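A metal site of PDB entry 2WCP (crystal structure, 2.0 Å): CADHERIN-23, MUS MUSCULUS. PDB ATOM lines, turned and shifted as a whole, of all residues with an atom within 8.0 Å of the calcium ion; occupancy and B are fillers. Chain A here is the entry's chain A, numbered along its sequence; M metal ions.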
ATOM      1  N   VAL A   3      31.590 -21.284  20.696  1.00  0.00           N
ATOM      2  CA  VAL A   3      32.148 -21.158  22.021  1.00  0.00           C
ATOM      3  C   VAL A   3      31.184 -20.192  22.762  1.00  0.00           C
ATOM      4  O   VAL A   3      30.580 -19.318  22.159  1.00  0.00           O
ATOM      5  CB  VAL A   3      33.629 -20.681  22.071  1.00  0.00           C
ATOM      6  CG1 VAL A   3      34.477 -21.487  21.061  1.00  0.00           C
ATOM      7  CG2 VAL A   3      33.752 -19.178  21.856  1.00  0.00           C
ATOM      8  N   ASN A   4      30.965 -20.488  24.014  1.00  0.00           N
ATOM      9  CA  ASN A   4      30.224 -19.595  24.900  1.00  0.00           C
ATOM     10  C   ASN A   4      30.700 -18.171  24.771  1.00  0.00           C
ATOM     11  O   ASN A   4      31.904 -17.943  24.734  1.00  0.00           O
ATOM     12  CB  ASN A   4      30.405 -20.042  26.345  1.00  0.00           C
ATOM     13  CG  ASN A   4      29.670 -19.132  27.319  1.00  0.00           C
ATOM     14  OD1 ASN A   4      28.480 -18.844  27.131  1.00  0.00           O
ATOM     15  ND2 ASN A   4      30.359 -18.687  28.372  1.00  0.00           N
ATOM     16  N   ARG A   5      29.763 -17.232  24.730  1.00  0.00           N
ATOM     17  CA  ARG A   5      30.065 -15.799  24.831  1.00  0.00           C
ATOM     18  C   ARG A   5      29.822 -15.348  26.290  1.00  0.00           C
ATOM     19  O   ARG A   5      28.731 -15.521  26.856  1.00  0.00           O
ATOM     20  CB  ARG A   5      29.222 -14.995  23.823  1.00  0.00           C
ATOM     21  CG  ARG A   5      29.447 -15.461  22.332  1.00  0.00           C
ATOM     22  CD  ARG A   5      28.426 -14.901  21.353  1.00  0.00           C
ATOM     23  NE  ARG A   5      27.139 -15.584  21.439  1.00  0.00           N
ATOM     24  CZ  ARG A   5      26.102 -15.340  20.641  1.00  0.00           C
ATOM     25  NH1 ARG A   5      24.982 -16.046  20.793  1.00  0.00           N
ATOM     26  NH2 ARG A   5      26.167 -14.425  19.681  1.00  0.00           N
ATOM     27  N   LEU A   6      30.872 -14.824  26.918  1.00  0.00           N
ATOM     28  CA  LEU A   6      30.772 -14.355  28.277  1.00  0.00           C
ATOM     29  C   LEU A   6      29.935 -13.080  28.332  1.00  0.00           C
ATOM     30  O   LEU A   6      29.809 -12.332  27.358  1.00  0.00           O
ATOM     31  CB  LEU A   6      32.156 -14.111  28.886  1.00  0.00           C
ATOM     32  CG  LEU A   6      32.996 -15.352  29.185  1.00  0.00           C
ATOM     33  CD1 LEU A   6      34.339 -14.939  29.837  1.00  0.00           C
ATOM     34  CD2 LEU A   6      32.254 -16.367  30.074  1.00  0.00           C
ATOM     35  N   PRO A   7      29.333 -12.853  29.489  1.00  0.00           N
ATOM     36  CA  PRO A   7      28.610 -11.619  29.686  1.00  0.00           C
ATOM     37  C   PRO A   7      29.546 -10.424  29.767  1.00  0.00           C
ATOM     38  O   PRO A   7      30.756 -10.579  30.005  1.00  0.00           O
ATOM     39  CB  PRO A   7      27.889 -11.850  31.001  1.00  0.00           C
ATOM     40  CG  PRO A   7      28.708 -12.816  31.727  1.00  0.00           C
ATOM     41  CD  PRO A   7      29.272 -13.732  30.666  1.00  0.00           C
ATOM     42  N   ARG A  36      24.845  -7.888  29.657  1.00  0.00           N
ATOM     43  CA  ARG A  36      24.260  -8.612  28.528  1.00  0.00           C
ATOM     44  C   ARG A  36      25.078  -9.859  28.272  1.00  0.00           C
ATOM     45  O   ARG A  36      26.304  -9.861  28.393  1.00  0.00           O
ATOM     46  CB  ARG A  36      24.186  -7.717  27.271  1.00  0.00           C
ATOM     47  CG  ARG A  36      23.732  -8.419  25.960  1.00  0.00           C
ATOM     48  CD  ARG A  36      22.281  -8.979  26.006  1.00  0.00           C
ATOM     49  NE  ARG A  36      21.929  -9.662  24.753  1.00  0.00           N
ATOM     50  CZ  ARG A  36      21.002 -10.624  24.645  1.00  0.00           C
ATOM     51  NH1 ARG A  36      20.332 -11.039  25.709  1.00  0.00           N
ATOM     52  NH2 ARG A  36      20.758 -11.163  23.474  1.00  0.00           N
ATOM     53  N   ASP A  37      24.372 -10.941  27.948  1.00  0.00           N
ATOM     54  CA  ASP A  37      24.980 -12.188  27.488  1.00  0.00           C
ATOM     55  C   ASP A  37      24.294 -12.523  26.171  1.00  0.00           C
ATOM     56  O   ASP A  37      23.086 -12.801  26.122  1.00  0.00           O
ATOM     57  CB  ASP A  37      24.786 -13.290  28.521  1.00  0.00           C
ATOM     58  CG  ASP A  37      25.550 -14.558  28.181  1.00  0.00           C
ATOM     59  OD1 ASP A  37      26.457 -14.970  28.957  1.00  0.00           O
ATOM     60  OD2 ASP A  37      25.206 -15.168  27.137  1.00  0.00           O
ATOM     61  N   MET A  38      25.076 -12.520  25.102  1.00  0.00           N
ATOM     62  CA  MET A  38      24.495 -12.673  23.766  1.00  0.00           C
ATOM     63  C   MET A  38      23.941 -14.083  23.523  1.00  0.00           C
ATOM     64  O   MET A  38      23.163 -14.297  22.573  1.00  0.00           O
ATOM     65  CB  MET A  38      25.510 -12.262  22.697  1.00  0.00           C
ATOM     66  CG  MET A  38      25.767 -10.753  22.626  1.00  0.00           C
ATOM     67  SD  MET A  38      24.241  -9.790  22.630  1.00  0.00           S
ATOM     68  CE  MET A  38      23.679 -10.031  20.953  1.00  0.00           C
ATOM     69  N   ASP A  39      24.283 -15.051  24.392  1.00  0.00           N
ATOM     70  CA  ASP A  39      23.647 -16.372  24.352  1.00  0.00           C
ATOM     71  C   ASP A  39      22.300 -16.370  25.103  1.00  0.00           C
ATOM     72  O   ASP A  39      21.608 -17.382  25.098  1.00  0.00           O
ATOM     73  CB  ASP A  39      24.524 -17.444  25.008  1.00  0.00           C
ATOM     74  CG  ASP A  39      25.930 -17.448  24.473  1.00  0.00           C
ATOM     75  OD1 ASP A  39      26.089 -17.494  23.242  1.00  0.00           O
ATOM     76  OD2 ASP A  39      26.885 -17.413  25.272  1.00  0.00           O
ATOM     77  N   ASN A  40      21.952 -15.260  25.755  1.00  0.00           N
ATOM     78  CA  ASN A  40      20.761 -15.177  26.617  1.00  0.00           C
ATOM     79  C   ASN A  40      20.862 -16.137  27.802  1.00  0.00           C
ATOM     80  O   ASN A  40      19.858 -16.632  28.298  1.00  0.00           O
ATOM     81  CB  ASN A  40      19.475 -15.402  25.782  1.00  0.00           C
ATOM     82  CG  ASN A  40      19.299 -14.351  24.707  1.00  0.00           C
ATOM     83  OD1 ASN A  40      19.650 -13.184  24.929  1.00  0.00           O
ATOM     84  ND2 ASN A  40      18.729 -14.736  23.547  1.00  0.00           N
ATOM     85  N   ASP A  41      22.089 -16.397  28.265  1.00  0.00           N
ATOM     86  CA  ASP A  41      22.292 -17.244  29.440  1.00  0.00           C
ATOM     87  C   ASP A  41      21.834 -16.496  30.682  1.00  0.00           C
ATOM     88  O   ASP A  41      22.048 -15.272  30.793  1.00  0.00           O
ATOM     89  CB  ASP A  41      23.778 -17.560  29.650  1.00  0.00           C
ATOM     90  CG  ASP A  41      24.349 -18.472  28.583  1.00  0.00           C
ATOM     91  OD1 ASP A  41      23.609 -19.315  28.055  1.00  0.00           O
ATOM     92  OD2 ASP A  41      25.547 -18.334  28.295  1.00  0.00           O
ATOM     93  N   PRO A  42      21.222 -17.218  31.647  1.00  0.00           N
ATOM     94  CA  PRO A  42      20.970 -16.587  32.953  1.00  0.00           C
ATOM     95  C   PRO A  42      22.261 -16.152  33.636  1.00  0.00           C
ATOM     96  O   PRO A  42      23.267 -16.841  33.546  1.00  0.00           O
ATOM     97  CB  PRO A  42      20.300 -17.700  33.774  1.00  0.00           C
ATOM     98  CG  PRO A  42      20.313 -18.907  32.959  1.00  0.00           C
ATOM     99  CD  PRO A  42      20.656 -18.568  31.544  1.00  0.00           C
ATOM    100  N   LEU A  43      22.221 -14.986  34.288  1.00  0.00           N
ATOM    101  CA  LEU A  43      23.412 -14.395  34.843  1.00  0.00           C
ATOM    102  C   LEU A  43      23.311 -14.272  36.352  1.00  0.00           C
ATOM    103  O   LEU A  43      22.210 -14.072  36.910  1.00  0.00           O
ATOM    104  CB  LEU A  43      23.671 -13.014  34.249  1.00  0.00           C
ATOM    105  CG  LEU A  43      23.874 -12.954  32.734  1.00  0.00           C
ATOM    106  CD1 LEU A  43      24.105 -11.518  32.291  1.00  0.00           C
ATOM    107  CD2 LEU A  43      25.013 -13.883  32.261  1.00  0.00           C
ATOM    108  N   SER A  86      28.470 -13.505  35.921  1.00  0.00           N
ATOM    109  CA  SER A  86      28.836 -14.877  35.456  1.00  0.00           C
ATOM    110  C   SER A  86      27.657 -15.503  34.774  1.00  0.00           C
ATOM    111  O   SER A  86      26.532 -15.335  35.212  1.00  0.00           O
ATOM    112  CB  SER A  86      29.238 -15.751  36.631  1.00  0.00           C
ATOM    113  OG  SER A  86      29.383 -17.108  36.234  1.00  0.00           O
ATOM    114  N   ASP A  87      27.929 -16.259  33.702  1.00  0.00           N
ATOM    115  CA  ASP A  87      26.880 -17.050  33.062  1.00  0.00           C
ATOM    116  C   ASP A  87      27.049 -18.525  33.448  1.00  0.00           C
ATOM    117  O   ASP A  87      26.530 -19.420  32.760  1.00  0.00           O
ATOM    118  CB  ASP A  87      26.935 -16.902  31.526  1.00  0.00           C
ATOM    119  CG  ASP A  87      28.279 -17.357  30.914  1.00  0.00           C
ATOM    120  OD1 ASP A  87      29.207 -17.808  31.660  1.00  0.00           O
ATOM    121  OD2 ASP A  87      28.400 -17.231  29.662  1.00  0.00           O
ATOM    122  N   HIS A  88      27.753 -18.756  34.550  1.00  0.00           N
ATOM    123  CA  HIS A  88      28.002 -20.101  35.116  1.00  0.00           C
ATOM    124  C   HIS A  88      29.051 -20.919  34.344  1.00  0.00           C
ATOM    125  O   HIS A  88      29.380 -22.012  34.759  1.00  0.00           O
ATOM    126  CB  HIS A  88      26.733 -20.932  35.298  1.00  0.00           C
ATOM    127  CG  HIS A  88      25.693 -20.301  36.165  1.00  0.00           C
ATOM    128  ND1 HIS A  88      25.853 -20.149  37.526  1.00  0.00           N
ATOM    129  CD2 HIS A  88      24.467 -19.806  35.874  1.00  0.00           C
ATOM    130  CE1 HIS A  88      24.765 -19.601  38.038  1.00  0.00           C
ATOM    131  NE2 HIS A  88      23.918 -19.362  37.050  1.00  0.00           N
ATOM    132  N   GLN A  89      29.583 -20.364  33.267  1.00  0.00           N
ATOM    133  CA  GLN A  89      30.671 -20.947  32.524  1.00  0.00           C
ATOM    134  C   GLN A  89      31.947 -20.124  32.713  1.00  0.00           C
ATOM    135  O   GLN A  89      33.044 -20.669  32.702  1.00  0.00           O
ATOM    136  CB  GLN A  89      30.246 -21.023  31.052  1.00  0.00           C
ATOM    137  CG  GLN A  89      28.908 -21.749  30.890  1.00  0.00           C
ATOM    138  CD  GLN A  89      28.074 -21.226  29.749  1.00  0.00           C
ATOM    139  OE1 GLN A  89      27.039 -20.525  29.949  1.00  0.00           O
ATOM    140  NE2 GLN A  89      28.520 -21.550  28.525  1.00  0.00           N
ATOM    141  N   GLY A  90      31.780 -18.813  32.897  1.00  0.00           N
ATOM    142  CA  GLY A  90      32.905 -17.941  33.196  1.00  0.00           C
ATOM    143  C   GLY A  90      32.434 -16.775  34.052  1.00  0.00           C
ATOM    144  O   GLY A  90      31.242 -16.523  34.154  1.00  0.00           O
HETATM  145 CA    CA M   1      27.155 -16.857  27.707  1.00  0.00          CA
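Of the 18 residues printed, 6 come within 4 Å of the calcium ion.
NH1 of Arg 5 lies within hydrogen-bond range of O of Met 38, at 3.1 Å.
OD2 of Asp 41 sits close to OE1 of Gln 89 (3.1 Å).
The side-chain carboxylate of Asp 87 sits at hydrogen-bond distance from the backbone NH of Gln 89 (3.0 Å).
N of Gly 90 sits at hydrogen-bond distance from OD1 of Asp 87, 3.0 Å away.
The side-chain amide nitrogen (ND2) of Asn 4 sits close to the side-chain amide nitrogen (NE2) of Gln 89, at 3.4 Å.
The calcium ion is bound by O of Arg 5 (2.2 Å), OD2 of Asp 41 (2.3 Å), OD2 of Asp 87 (2.3 Å), OD1 of Asp 37 (2.4 Å), OD1 of Asn 4 (2.5 Å), OD2 of Asp 39 (2.5 Å) and OD2 of Asp 37 (2.6 Å).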
